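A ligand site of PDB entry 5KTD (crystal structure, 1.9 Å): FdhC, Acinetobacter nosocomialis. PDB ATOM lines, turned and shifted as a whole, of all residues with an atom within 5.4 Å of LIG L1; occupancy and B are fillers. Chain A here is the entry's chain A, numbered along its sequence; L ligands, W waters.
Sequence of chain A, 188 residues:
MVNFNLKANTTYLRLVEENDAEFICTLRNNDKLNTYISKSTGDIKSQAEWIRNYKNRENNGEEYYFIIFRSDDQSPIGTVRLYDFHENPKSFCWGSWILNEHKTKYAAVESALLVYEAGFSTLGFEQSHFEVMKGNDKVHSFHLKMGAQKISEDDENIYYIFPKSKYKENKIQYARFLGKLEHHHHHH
OH of Tyr 174 is in hydrogen-bond range of N3 of LIG L1, at 2.6 Å.
N7 of LIG L1 lies within hydrogen-bond range of O of Trp 97 (2.6 Å).
O9 of LIG L1 is in salt-bridge range of NZ of Lys 138, at 2.8 Å.
O11 of LIG L1 is in salt-bridge range of NZ of Lys 103, at 2.8 Å.
An oxygen (O3) of LIG L1 lies within salt-bridge range of the side-chain amino group (NZ) of Lys 105 (2.9 Å).
O15 of LIG L1 lies within hydrogen-bond range of N of Leu 99 (2.9 Å).
O16 of LIG L1 sits at hydrogen-bond distance from ND2 of Asn 136 (3.0 Å).
The backbone carbonyl oxygen (O) of Glu 131 sits at hydrogen-bond distance from a nitrogen (N1) of LG2 L2, 3.2 Å away.
O of Tyr 36 lies within hydrogen-bond range of O3 of LG2 L2 (3.4 Å).
A sulfur (S1) of LIG L1 lies close to an oxygen (O2) of LG2 L2, 3.2 Å away.
Residues that only touch LIG L1: Leu 33, Ile 37, Ile 98, Tyr 106, Ala 108, Val 109, Glu 131, Val 132, Val 139, Phe 142 and Lys 145.
Hydrophobic or aromatic side chains that line LIG L1: Ile 37, Trp 97, Ile 98, Leu 99, Tyr 106, Ala 108, Val 109, Val 132, Val 139, Phe 142 and Tyr 174.
18 residues have an atom within 4 Å of LIG L1: Leu 33, Ile 37, Trp 97, Ile 98, Leu 99, Lys 103, Lys 105, Tyr 106, Ala 108, Val 109, Glu 131, Val 132, Asn 136, Lys 138, Val 139, Phe 142, Lys 145 and Tyr 174.
The nearest printed residue that does not touch LIG L1 is Tyr 36 (4.01 Å).
Water W5 lies within hydrogen-bond range of an oxygen (O8) of LIG L1 and the backbone carbonyl oxygen (O) of Lys 138.
Water W3 lies within hydrogen-bond range of an oxygen (O11) of LIG L1 (2.8 Å), the backbone carbonyl oxygen (O) of Lys 105 (2.9 Å) and the backbone NH (N) of Ala 108 (2.9 Å).
Water W7 lies within hydrogen-bond range of the backbone NH (N) of Tyr 36 (2.7 Å), the backbone carbonyl oxygen (O) of Leu 33 (2.8 Å) and an oxygen (O16) of LIG L1 (2.9 Å).
Water W2 lies within hydrogen-bond range of the backbone carbonyl oxygen (O) of Phe 142 and a nitrogen (N4) of LIG L1.
Water W6 bridges OD1 of Asn 136 (2.7 Å) and N6 of LIG L1 (3.1 Å).
Water W1 lies within hydrogen-bond range of N of Met 133 (2.8 Å), O of Tyr 36 (2.9 Å), O3 of LG2 L2 (3.0 Å), S1 of LIG L1 (3.1 Å) and ND2 of Asn 136 (3.2 Å).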
ATOM      1  N   LEU A  33       5.170 -25.403 -28.306  1.00  0.00           N
ATOM      2  CA  LEU A  33       3.976 -25.717 -27.530  1.00  0.00           C
ATOM      3  C   LEU A  33       3.723 -27.185 -27.297  1.00  0.00           C
ATOM      4  O   LEU A  33       2.948 -27.500 -26.426  1.00  0.00           O
ATOM      5  CB  LEU A  33       2.731 -25.151 -28.256  1.00  0.00           C
ATOM      6  CG  LEU A  33       2.743 -23.627 -28.446  1.00  0.00           C
ATOM      7  CD1 LEU A  33       1.490 -23.188 -29.188  1.00  0.00           C
ATOM      8  CD2 LEU A  33       2.896 -22.870 -27.104  1.00  0.00           C
ATOM      9  N   ASN A  34       4.343 -28.064 -28.064  1.00  0.00           N
ATOM     10  CA  ASN A  34       3.873 -29.429 -28.132  1.00  0.00           C
ATOM     11  C   ASN A  34       4.760 -30.433 -27.430  1.00  0.00           C
ATOM     12  O   ASN A  34       4.592 -31.633 -27.639  1.00  0.00           O
ATOM     13  CB  ASN A  34       3.601 -29.878 -29.549  1.00  0.00           C
ATOM     14  CG  ASN A  34       4.857 -29.988 -30.422  1.00  0.00           C
ATOM     15  OD1 ASN A  34       5.994 -29.843 -29.972  1.00  0.00           O
ATOM     16  ND2 ASN A  34       4.635 -30.242 -31.699  1.00  0.00           N
ATOM     17  N   TYR A  36       4.842 -31.560 -24.421  1.00  0.00           N
ATOM     18  CA  TYR A  36       4.217 -32.448 -23.476  1.00  0.00           C
ATOM     19  C   TYR A  36       2.814 -32.918 -23.917  1.00  0.00           C
ATOM     20  O   TYR A  36       2.040 -33.360 -23.067  1.00  0.00           O
ATOM     21  CB  TYR A  36       4.155 -31.729 -22.114  1.00  0.00           C
ATOM     22  CG  TYR A  36       5.523 -31.384 -21.583  1.00  0.00           C
ATOM     23  CD1 TYR A  36       6.417 -32.375 -21.180  1.00  0.00           C
ATOM     24  CD2 TYR A  36       5.928 -30.063 -21.479  1.00  0.00           C
ATOM     25  CE1 TYR A  36       7.660 -32.069 -20.695  1.00  0.00           C
ATOM     26  CE2 TYR A  36       7.174 -29.728 -20.994  1.00  0.00           C
ATOM     27  CZ  TYR A  36       8.050 -30.725 -20.606  1.00  0.00           C
ATOM     28  OH  TYR A  36       9.278 -30.382 -20.089  1.00  0.00           O
ATOM     29  N   ILE A  37       2.481 -32.836 -25.209  1.00  0.00           N
ATOM     30  CA  ILE A  37       1.153 -33.298 -25.654  1.00  0.00           C
ATOM     31  C   ILE A  37       1.381 -34.371 -26.684  1.00  0.00           C
ATOM     32  O   ILE A  37       2.511 -34.582 -27.068  1.00  0.00           O
ATOM     33  CB  ILE A  37       0.280 -32.153 -26.186  1.00  0.00           C
ATOM     34  CG1 ILE A  37       0.832 -31.593 -27.491  1.00  0.00           C
ATOM     35  CG2 ILE A  37       0.204 -31.065 -25.116  1.00  0.00           C
ATOM     36  CD1 ILE A  37       0.034 -30.462 -28.096  1.00  0.00           C
ATOM     37  N   TRP A  97      -5.052 -28.928 -23.936  1.00  0.00           N
ATOM     38  CA  TRP A  97      -5.097 -27.561 -23.430  1.00  0.00           C
ATOM     39  C   TRP A  97      -3.816 -26.834 -23.879  1.00  0.00           C
ATOM     40  O   TRP A  97      -2.724 -27.125 -23.393  1.00  0.00           O
ATOM     41  CB  TRP A  97      -5.185 -27.584 -21.936  1.00  0.00           C
ATOM     42  CG  TRP A  97      -5.448 -26.261 -21.293  1.00  0.00           C
ATOM     43  CD1 TRP A  97      -6.258 -25.249 -21.734  1.00  0.00           C
ATOM     44  CD2 TRP A  97      -4.952 -25.860 -20.027  1.00  0.00           C
ATOM     45  NE1 TRP A  97      -6.242 -24.212 -20.816  1.00  0.00           N
ATOM     46  CE2 TRP A  97      -5.477 -24.580 -19.756  1.00  0.00           C
ATOM     47  CE3 TRP A  97      -4.095 -26.478 -19.080  1.00  0.00           C
ATOM     48  CZ2 TRP A  97      -5.173 -23.886 -18.602  1.00  0.00           C
ATOM     49  CZ3 TRP A  97      -3.787 -25.777 -17.919  1.00  0.00           C
ATOM     50  CH2 TRP A  97      -4.326 -24.481 -17.704  1.00  0.00           C
ATOM     51  N   ILE A  98      -4.002 -25.912 -24.818  1.00  0.00           N
ATOM     52  CA  ILE A  98      -2.918 -25.283 -25.509  1.00  0.00           C
ATOM     53  C   ILE A  98      -3.299 -23.818 -25.701  1.00  0.00           C
ATOM     54  O   ILE A  98      -4.440 -23.515 -26.079  1.00  0.00           O
ATOM     55  CB  ILE A  98      -2.612 -25.874 -26.891  1.00  0.00           C
ATOM     56  CG1 ILE A  98      -2.428 -27.401 -26.852  1.00  0.00           C
ATOM     57  CG2 ILE A  98      -1.322 -25.255 -27.372  1.00  0.00           C
ATOM     58  CD1 ILE A  98      -2.615 -28.085 -28.207  1.00  0.00           C
ATOM     59  N   LEU A  99      -2.364 -22.932 -25.396  1.00  0.00           N
ATOM     60  CA  LEU A  99      -2.515 -21.486 -25.663  1.00  0.00           C
ATOM     61  C   LEU A  99      -1.265 -20.978 -26.379  1.00  0.00           C
ATOM     62  O   LEU A  99      -0.150 -21.335 -25.976  1.00  0.00           O
ATOM     63  CB  LEU A  99      -2.685 -20.758 -24.346  1.00  0.00           C
ATOM     64  CG  LEU A  99      -3.990 -20.885 -23.583  1.00  0.00           C
ATOM     65  CD1 LEU A  99      -3.872 -20.288 -22.191  1.00  0.00           C
ATOM     66  CD2 LEU A  99      -5.153 -20.248 -24.335  1.00  0.00           C
ATOM     67  N   LYS A 103      -1.986 -15.310 -26.714  1.00  0.00           N
ATOM     68  CA  LYS A 103      -2.863 -15.445 -25.618  1.00  0.00           C
ATOM     69  C   LYS A 103      -2.863 -14.172 -24.755  1.00  0.00           C
ATOM     70  O   LYS A 103      -1.822 -13.516 -24.608  1.00  0.00           O
ATOM     71  CB  LYS A 103      -2.423 -16.630 -24.727  1.00  0.00           C
ATOM     72  CG  LYS A 103      -1.110 -16.400 -23.980  1.00  0.00           C
ATOM     73  CD  LYS A 103      -0.509 -17.685 -23.415  1.00  0.00           C
ATOM     74  CE  LYS A 103       0.712 -17.368 -22.523  1.00  0.00           C
ATOM     75  NZ  LYS A 103       1.519 -18.586 -22.220  1.00  0.00           N
ATOM     76  N   LYS A 105      -2.752 -12.561 -21.099  1.00  0.00           N
ATOM     77  CA  LYS A 105      -1.902 -12.950 -19.969  1.00  0.00           C
ATOM     78  C   LYS A 105      -2.498 -14.074 -19.085  1.00  0.00           C
ATOM     79  O   LYS A 105      -1.786 -15.000 -18.728  1.00  0.00           O
ATOM     80  CB  LYS A 105      -1.599 -11.739 -19.084  1.00  0.00           C
ATOM     81  CG  LYS A 105      -0.591 -12.021 -17.967  1.00  0.00           C
ATOM     82  CD  LYS A 105       0.161 -10.729 -17.634  1.00  0.00           C
ATOM     83  CE  LYS A 105       1.128 -10.879 -16.463  1.00  0.00           C
ATOM     84  NZ  LYS A 105       2.450 -11.392 -16.899  1.00  0.00           N
ATOM     85  N   TYR A 106      -3.785 -13.935 -18.740  1.00  0.00           N
ATOM     86  CA  TYR A 106      -4.491 -14.815 -17.804  1.00  0.00           C
ATOM     87  C   TYR A 106      -5.455 -15.806 -18.512  1.00  0.00           C
ATOM     88  O   TYR A 106      -6.344 -16.381 -17.863  1.00  0.00           O
ATOM     89  CB  TYR A 106      -5.273 -13.986 -16.756  1.00  0.00           C
ATOM     90  CG  TYR A 106      -4.322 -13.072 -15.990  1.00  0.00           C
ATOM     91  CD1 TYR A 106      -3.478 -13.582 -14.994  1.00  0.00           C
ATOM     92  CD2 TYR A 106      -4.210 -11.698 -16.295  1.00  0.00           C
ATOM     93  CE1 TYR A 106      -2.568 -12.764 -14.323  1.00  0.00           C
ATOM     94  CE2 TYR A 106      -3.284 -10.875 -15.638  1.00  0.00           C
ATOM     95  CZ  TYR A 106      -2.496 -11.408 -14.664  1.00  0.00           C
ATOM     96  OH  TYR A 106      -1.604 -10.624 -14.024  1.00  0.00           O
ATOM     97  N   ALA A 108      -5.004 -18.764 -19.394  1.00  0.00           N
ATOM     98  CA  ALA A 108      -4.905 -20.112 -18.781  1.00  0.00           C
ATOM     99  C   ALA A 108      -5.886 -20.217 -17.629  1.00  0.00           C
ATOM    100  O   ALA A 108      -6.659 -21.172 -17.544  1.00  0.00           O
ATOM    101  CB  ALA A 108      -3.486 -20.418 -18.351  1.00  0.00           C
ATOM    102  N   VAL A 109      -5.890 -19.206 -16.750  1.00  0.00           N
ATOM    103  CA  VAL A 109      -6.837 -19.193 -15.617  1.00  0.00           C
ATOM    104  C   VAL A 109      -8.270 -19.142 -16.127  1.00  0.00           C
ATOM    105  O   VAL A 109      -9.173 -19.865 -15.624  1.00  0.00           O
ATOM    106  CB  VAL A 109      -6.623 -18.023 -14.606  1.00  0.00           C
ATOM    107  CG1 VAL A 109      -7.635 -18.104 -13.478  1.00  0.00           C
ATOM    108  CG2 VAL A 109      -5.216 -17.986 -14.050  1.00  0.00           C
ATOM    109  N   GLU A 131      -4.416 -35.535 -16.455  1.00  0.00           N
ATOM    110  CA  GLU A 131      -3.047 -35.843 -16.182  1.00  0.00           C
ATOM    111  C   GLU A 131      -2.147 -34.850 -16.860  1.00  0.00           C
ATOM    112  O   GLU A 131      -2.570 -34.185 -17.786  1.00  0.00           O
ATOM    113  CB  GLU A 131      -2.720 -37.270 -16.640  1.00  0.00           C
ATOM    114  CG  GLU A 131      -2.731 -37.557 -18.123  1.00  0.00           C
ATOM    115  CD  GLU A 131      -4.015 -38.158 -18.616  1.00  0.00           C
ATOM    116  OE1 GLU A 131      -4.393 -37.937 -19.766  1.00  0.00           O
ATOM    117  OE2 GLU A 131      -4.646 -38.890 -17.881  1.00  0.00           O
ATOM    118  N   VAL A 132      -0.906 -34.792 -16.406  1.00  0.00           N
ATOM    119  CA  VAL A 132       0.068 -33.834 -16.871  1.00  0.00           C
ATOM    120  C   VAL A 132       1.387 -34.579 -16.886  1.00  0.00           C
ATOM    121  O   VAL A 132       1.699 -35.263 -15.910  1.00  0.00           O
ATOM    122  CB  VAL A 132       0.200 -32.693 -15.863  1.00  0.00           C
ATOM    123  CG1 VAL A 132       1.286 -31.694 -16.260  1.00  0.00           C
ATOM    124  CG2 VAL A 132      -1.175 -32.013 -15.622  1.00  0.00           C
ATOM    125  N   MET A 133       2.132 -34.468 -17.977  1.00  0.00           N
ATOM    126  CA  MET A 133       3.458 -35.107 -18.046  1.00  0.00           C
ATOM    127  C   MET A 133       4.415 -34.683 -16.982  1.00  0.00           C
ATOM    128  O   MET A 133       4.536 -33.514 -16.699  1.00  0.00           O
ATOM    129  CB  MET A 133       4.139 -34.886 -19.391  1.00  0.00           C
ATOM    130  CG  MET A 133       3.487 -35.741 -20.478  1.00  0.00           C
ATOM    131  SD  MET A 133       4.481 -35.951 -21.974  1.00  0.00           S
ATOM    132  CE  MET A 133       5.763 -37.053 -21.355  1.00  0.00           C
ATOM    133  N   ASN A 136       6.531 -31.245 -17.185  1.00  0.00           N
ATOM    134  CA  ASN A 136       5.726 -30.049 -17.482  1.00  0.00           C
ATOM    135  C   ASN A 136       5.443 -29.205 -16.240  1.00  0.00           C
ATOM    136  O   ASN A 136       4.284 -28.976 -15.827  1.00  0.00           O
ATOM    137  CB  ASN A 136       4.438 -30.479 -18.184  1.00  0.00           C
ATOM    138  CG  ASN A 136       3.838 -29.401 -19.092  1.00  0.00           C
ATOM    139  OD1 ASN A 136       4.263 -28.253 -19.128  1.00  0.00           O
ATOM    140  ND2 ASN A 136       2.851 -29.823 -19.862  1.00  0.00           N
ATOM    141  N   LYS A 138       5.391 -26.194 -14.715  1.00  0.00           N
ATOM    142  CA  LYS A 138       4.519 -25.097 -14.416  1.00  0.00           C
ATOM    143  C   LYS A 138       3.020 -25.507 -14.478  1.00  0.00           C
ATOM    144  O   LYS A 138       2.172 -24.844 -13.903  1.00  0.00           O
ATOM    145  CB  LYS A 138       4.817 -23.947 -15.428  1.00  0.00           C
ATOM    146  CG  LYS A 138       4.337 -22.606 -14.997  1.00  0.00           C
ATOM    147  CD  LYS A 138       4.706 -21.497 -15.988  1.00  0.00           C
ATOM    148  CE  LYS A 138       4.354 -20.159 -15.327  1.00  0.00           C
ATOM    149  NZ  LYS A 138       4.210 -18.979 -16.222  1.00  0.00           N
ATOM    150  N   VAL A 139       2.709 -26.576 -15.215  1.00  0.00           N
ATOM    151  CA  VAL A 139       1.303 -27.045 -15.375  1.00  0.00           C
ATOM    152  C   VAL A 139       0.867 -27.763 -14.074  1.00  0.00           C
ATOM    153  O   VAL A 139      -0.215 -27.505 -13.500  1.00  0.00           O
ATOM    154  CB  VAL A 139       1.161 -27.873 -16.678  1.00  0.00           C
ATOM    155  CG1 VAL A 139      -0.272 -28.411 -16.860  1.00  0.00           C
ATOM    156  CG2 VAL A 139       1.573 -26.996 -17.869  1.00  0.00           C
ATOM    157  N   PHE A 142       0.341 -25.022 -11.704  1.00  0.00           N
ATOM    158  CA  PHE A 142      -0.984 -24.419 -11.940  1.00  0.00           C
ATOM    159  C   PHE A 142      -2.170 -25.174 -11.325  1.00  0.00           C
ATOM    160  O   PHE A 142      -3.052 -24.586 -10.713  1.00  0.00           O
ATOM    161  CB  PHE A 142      -1.240 -24.309 -13.476  1.00  0.00           C
ATOM    162  CG  PHE A 142      -2.556 -23.679 -13.839  1.00  0.00           C
ATOM    163  CD1 PHE A 142      -3.741 -24.408 -13.877  1.00  0.00           C
ATOM    164  CD2 PHE A 142      -2.605 -22.327 -14.203  1.00  0.00           C
ATOM    165  CE1 PHE A 142      -4.945 -23.808 -14.207  1.00  0.00           C
ATOM    166  CE2 PHE A 142      -3.794 -21.722 -14.548  1.00  0.00           C
ATOM    167  CZ  PHE A 142      -4.978 -22.472 -14.532  1.00  0.00           C
ATOM    168  N   LYS A 145      -2.163 -25.278  -7.473  1.00  0.00           N
ATOM    169  CA  LYS A 145      -2.641 -23.986  -7.006  1.00  0.00           C
ATOM    170  C   LYS A 145      -4.163 -23.813  -7.082  1.00  0.00           C
ATOM    171  O   LYS A 145      -4.797 -23.288  -6.135  1.00  0.00           O
ATOM    172  CB  LYS A 145      -1.894 -22.889  -7.774  1.00  0.00           C
ATOM    173  CG  LYS A 145      -2.124 -21.476  -7.244  1.00  0.00           C
ATOM    174  CD  LYS A 145      -0.983 -20.554  -7.700  1.00  0.00           C
ATOM    175  CE  LYS A 145      -1.301 -19.057  -7.617  1.00  0.00           C
ATOM    176  NZ  LYS A 145      -2.077 -18.739  -6.388  1.00  0.00           N
ATOM    177  N   MET A 146      -4.780 -24.260  -8.170  1.00  0.00           N
ATOM    178  CA  MET A 146      -6.250 -24.134  -8.318  1.00  0.00           C
ATOM    179  C   MET A 146      -7.062 -25.099  -7.453  1.00  0.00           C
ATOM    180  O   MET A 146      -8.237 -24.905  -7.259  1.00  0.00           O
ATOM    181  CB  MET A 146      -6.688 -24.314  -9.789  1.00  0.00           C
ATOM    182  CG  MET A 146      -8.121 -23.865 -10.083  1.00  0.00           C
ATOM    183  SD  MET A 146      -8.334 -23.752 -11.864  1.00  0.00           S
ATOM    184  CE  MET A 146      -7.458 -22.239 -12.239  1.00  0.00           C
ATOM    185  N   TYR A 174     -12.310 -16.778  -7.545  1.00  0.00           N
ATOM    186  CA  TYR A 174     -11.812 -16.505  -8.890  1.00  0.00           C
ATOM    187  C   TYR A 174     -12.791 -15.650  -9.742  1.00  0.00           C
ATOM    188  O   TYR A 174     -12.570 -15.480 -10.949  1.00  0.00           O
ATOM    189  CB  TYR A 174     -11.517 -17.845  -9.580  1.00  0.00           C
ATOM    190  CG  TYR A 174     -10.214 -18.481  -9.124  1.00  0.00           C
ATOM    191  CD1 TYR A 174     -10.158 -19.313  -8.006  1.00  0.00           C
ATOM    192  CD2 TYR A 174      -9.072 -18.197  -9.791  1.00  0.00           C
ATOM    193  CE1 TYR A 174      -8.954 -19.898  -7.582  1.00  0.00           C
ATOM    194  CE2 TYR A 174      -7.863 -18.761  -9.408  1.00  0.00           C
ATOM    195  CZ  TYR A 174      -7.822 -19.628  -8.291  1.00  0.00           C
ATOM    196  OH  TYR A 174      -6.619 -20.134  -7.933  1.00  0.00           O
ATOM    197  N   ARG A 176     -13.163 -12.539 -10.299  1.00  0.00           N
ATOM    198  CA  ARG A 176     -12.535 -11.460 -11.106  1.00  0.00           C
ATOM    199  C   ARG A 176     -12.045 -11.953 -12.491  1.00  0.00           C
ATOM    200  O   ARG A 176     -11.831 -11.129 -13.454  1.00  0.00           O
ATOM    201  CB  ARG A 176     -11.384 -10.797 -10.386  1.00  0.00           C
ATOM    202  CG  ARG A 176     -10.149 -11.627 -10.281  1.00  0.00           C
ATOM    203  CD  ARG A 176      -9.181 -10.891  -9.444  1.00  0.00           C
ATOM    204  NE  ARG A 176      -8.169 -11.765  -8.950  1.00  0.00           N
ATOM    205  CZ  ARG A 176      -6.980 -11.904  -9.507  1.00  0.00           C
ATOM    206  NH1 ARG A 176      -6.688 -11.222 -10.610  1.00  0.00           N
ATOM    207  NH2 ARG A 176      -6.104 -12.744  -9.004  1.00  0.00           N
ATOM    208  N   PHE A 177     -11.799 -13.259 -12.597  1.00  0.00           N
ATOM    209  CA  PHE A 177     -11.336 -13.806 -13.863  1.00  0.00           C
ATOM    210  C   PHE A 177     -12.494 -14.099 -14.814  1.00  0.00           C
ATOM    211  O   PHE A 177     -12.288 -14.212 -16.025  1.00  0.00           O
ATOM    212  CB  PHE A 177     -10.538 -15.066 -13.620  1.00  0.00           C
ATOM    213  CG  PHE A 177      -9.192 -14.818 -13.020  1.00  0.00           C
ATOM    214  CD1 PHE A 177      -8.138 -14.385 -13.812  1.00  0.00           C
ATOM    215  CD2 PHE A 177      -8.974 -15.067 -11.659  1.00  0.00           C
ATOM    216  CE1 PHE A 177      -6.861 -14.209 -13.301  1.00  0.00           C
ATOM    217  CE2 PHE A 177      -7.724 -14.860 -11.118  1.00  0.00           C
ATOM    218  CZ  PHE A 177      -6.659 -14.429 -11.931  1.00  0.00           C
HETATM  219  N1  LIG L   1      -4.344 -17.580  -9.424  1.00  0.00           N
HETATM  220  C1  LIG L   1      -3.849 -16.410  -9.864  1.00  0.00           C
HETATM  221  N2  LIG L   1      -3.055 -16.318 -10.916  1.00  0.00           N
HETATM  222  C2  LIG L   1      -2.711 -17.407 -11.619  1.00  0.00           C
HETATM  223  C3  LIG L   1      -3.212 -18.718 -11.212  1.00  0.00           C
HETATM  224  C4  LIG L   1      -4.062 -18.741 -10.031  1.00  0.00           C
HETATM  225  N3  LIG L   1      -4.586 -19.888  -9.585  1.00  0.00           N
HETATM  226  N4  LIG L   1      -2.749 -19.633 -12.071  1.00  0.00           N
HETATM  227  C5  LIG L   1      -1.979 -18.957 -12.951  1.00  0.00           C
HETATM  228  N5  LIG L   1      -1.940 -17.618 -12.663  1.00  0.00           N
HETATM  229  C6  LIG L   1      -1.216 -16.582 -13.446  1.00  0.00           C
HETATM  230  C7  LIG L   1       0.214 -16.997 -13.764  1.00  0.00           C
HETATM  231  O1  LIG L   1       1.226 -16.648 -12.806  1.00  0.00           O
HETATM  232  C8  LIG L   1       0.447 -16.353 -15.107  1.00  0.00           C
HETATM  233  O2  LIG L   1       0.840 -14.988 -14.918  1.00  0.00           O
HETATM  234  P1  LIG L   1       2.423 -14.649 -15.046  1.00  0.00           P
HETATM  235  O3  LIG L   1       2.579 -14.290 -16.527  1.00  0.00           O
HETATM  236  O4  LIG L   1       2.488 -13.424 -14.152  1.00  0.00           O
HETATM  237  O5  LIG L   1       3.195 -15.863 -14.556  1.00  0.00           O
HETATM  238  C9  LIG L   1      -0.890 -16.425 -15.790  1.00  0.00           C
HETATM  239  O6  LIG L   1      -1.857 -16.523 -14.730  1.00  0.00           O
HETATM  240  C10 LIG L   1      -0.983 -17.576 -16.809  1.00  0.00           C
HETATM  241  O7  LIG L   1      -0.787 -18.841 -16.167  1.00  0.00           O
HETATM  242  P2  LIG L   1       0.392 -19.802 -16.639  1.00  0.00           P
HETATM  243  O8  LIG L   1       0.564 -20.836 -15.589  1.00  0.00           O
HETATM  244  O9  LIG L   1       1.628 -19.143 -17.195  1.00  0.00           O
HETATM  245  O10 LIG L   1      -0.279 -20.578 -17.878  1.00  0.00           O
HETATM  246  P3  LIG L   1       0.195 -20.573 -19.393  1.00  0.00           P
HETATM  247  O11 LIG L   1      -0.126 -19.249 -20.077  1.00  0.00           O
HETATM  248  O12 LIG L   1       1.496 -21.239 -19.654  1.00  0.00           O
HETATM  249  O13 LIG L   1      -0.869 -21.619 -20.019  1.00  0.00           O
HETATM  250  C11 LIG L   1      -0.778 -23.850 -20.865  1.00  0.00           C
HETATM  251  C12 LIG L   1      -0.757 -22.983 -19.614  1.00  0.00           C
HETATM  252  C13 LIG L   1      -0.610 -25.290 -20.395  1.00  0.00           C
HETATM  253  C14 LIG L   1      -2.121 -23.609 -21.549  1.00  0.00           C
HETATM  254  C15 LIG L   1       0.369 -23.440 -21.809  1.00  0.00           C
HETATM  255  O14 LIG L   1       1.588 -23.316 -21.055  1.00  0.00           O
HETATM  256  C16 LIG L   1       0.534 -24.345 -22.983  1.00  0.00           C
HETATM  257  O15 LIG L   1      -0.110 -24.179 -24.006  1.00  0.00           O
HETATM  258  N6  LIG L   1       1.454 -25.311 -22.840  1.00  0.00           N
HETATM  259  C17 LIG L   1       1.834 -26.198 -23.886  1.00  0.00           C
HETATM  260  C18 LIG L   1       0.812 -27.310 -24.121  1.00  0.00           C
HETATM  261  C19 LIG L   1       0.654 -28.145 -22.866  1.00  0.00           C
HETATM  262  O16 LIG L   1       1.656 -28.605 -22.306  1.00  0.00           O
HETATM  263  N7  LIG L   1      -0.585 -28.314 -22.407  1.00  0.00           N
HETATM  264  C20 LIG L   1      -0.892 -28.987 -21.148  1.00  0.00           C
HETATM  265  C21 LIG L   1      -0.806 -30.527 -21.197  1.00  0.00           C
HETATM  266  S1  LIG L   1      -0.894 -31.204 -19.509  1.00  0.00           S
HETATM  267  O1  LG2 L   2      -4.026 -31.160 -21.429  1.00  0.00           O
HETATM  268  C1  LG2 L   2      -4.056 -32.028 -20.537  1.00  0.00           C
HETATM  269  C2  LG2 L   2      -4.625 -31.826 -19.173  1.00  0.00           C
HETATM  270  C3  LG2 L   2      -4.743 -30.368 -18.817  1.00  0.00           C
HETATM  271  O2  LG2 L   2      -3.536 -29.902 -18.200  1.00  0.00           O
HETATM  272  C4  LG2 L   2      -5.826 -30.087 -17.814  1.00  0.00           C
HETATM  273  N1  LG2 L   2      -3.561 -33.306 -20.732  1.00  0.00           N
HETATM  274  C5  LG2 L   2      -3.188 -33.810 -22.056  1.00  0.00           C
HETATM  275  C6  LG2 L   2      -1.914 -34.650 -21.961  1.00  0.00           C
HETATM  276  O3  LG2 L   2      -0.869 -33.830 -21.382  1.00  0.00           O
HETATM  277  C7  LG2 L   2      -1.546 -35.090 -23.382  1.00  0.00           C
HETATM  278  C8  LG2 L   2      -0.256 -35.903 -23.449  1.00  0.00           C
HETATM  279  O4  LG2 L   2      -2.621 -35.872 -23.938  1.00  0.00           O
HETATM  280  C9  LG2 L   2      -4.245 -34.736 -22.595  1.00  0.00           C
HETATM  281  O5  LG2 L   2      -5.529 -34.150 -22.617  1.00  0.00           O
HETATM  282  C10 LG2 L   2      -3.897 -35.223 -23.954  1.00  0.00           C
HETATM  283  O6  LG2 L   2      -3.925 -34.116 -24.850  1.00  0.00           O
HETATM  284  P1  LG2 L   2      -3.967 -34.372 -26.380  1.00  0.00           P
HETATM  285  O7  LG2 L   2      -2.599 -34.697 -26.993  1.00  0.00           O
HETATM  286  O8  LG2 L   2      -4.655 -33.087 -26.944  1.00  0.00           O
HETATM  287  O9  LG2 L   2      -5.092 -35.413 -26.853  1.00  0.00           O
HETATM  288  P2  LG2 L   2      -5.066 -37.019 -26.830  1.00  0.00           P
HETATM  289  O10 LG2 L   2      -6.189 -37.595 -26.112  1.00  0.00           O
HETATM  290  O11 LG2 L   2      -3.735 -37.557 -26.306  1.00  0.00           O
HETATM  291  O12 LG2 L   2      -5.289 -37.366 -28.351  1.00  0.00           O
HETATM  292  C11 LG2 L   2      -5.745 -38.620 -28.842  1.00  0.00           C
HETATM  293  C12 LG2 L   2      -5.156 -38.738 -30.227  1.00  0.00           C
HETATM  294  C13 LG2 L   2      -3.646 -38.427 -30.268  1.00  0.00           C
HETATM  295  O13 LG2 L   2      -3.019 -39.250 -31.269  1.00  0.00           O
HETATM  296  C14 LG2 L   2      -3.536 -36.998 -30.803  1.00  0.00           C
HETATM  297  C15 LG2 L   2      -4.746 -36.932 -31.718  1.00  0.00           C
HETATM  298  O14 LG2 L   2      -5.762 -37.808 -31.145  1.00  0.00           O
HETATM  299  N2  LG2 L   2      -5.374 -35.636 -31.889  1.00  0.00           N
HETATM  300  C16 LG2 L   2      -5.963 -35.022 -30.812  1.00  0.00           C
HETATM  301  C17 LG2 L   2      -6.637 -33.801 -30.973  1.00  0.00           C
HETATM  302  C18 LG2 L   2      -7.330 -33.092 -29.829  1.00  0.00           C
HETATM  303  C19 LG2 L   2      -6.619 -33.231 -32.290  1.00  0.00           C
HETATM  304  O15 LG2 L   2      -7.214 -32.116 -32.522  1.00  0.00           O
HETATM  305  N3  LG2 L   2      -6.038 -33.852 -33.310  1.00  0.00           N
HETATM  306  C20 LG2 L   2      -5.438 -35.024 -33.129  1.00  0.00           C
HETATM  307  O16 LG2 L   2      -4.897 -35.556 -34.204  1.00  0.00           O
HETATM  308  O   HOH W   1       1.707 -32.791 -20.226  1.00  0.00           O
HETATM  309  O   HOH W   2      -3.858 -22.276 -11.319  1.00  0.00           O
HETATM  310  O   HOH W   3      -2.361 -17.616 -19.891  1.00  0.00           O
HETATM  311  O   HOH W   4       3.430 -22.571 -22.927  1.00  0.00           O
HETATM  312  O   HOH W   5       0.808 -23.285 -16.178  1.00  0.00           O
HETATM  313  O   HOH W   6       3.612 -26.214 -20.810  1.00  0.00           O
HETATM  314  O   HOH W   7       3.845 -29.011 -24.192  1.00  0.00           O
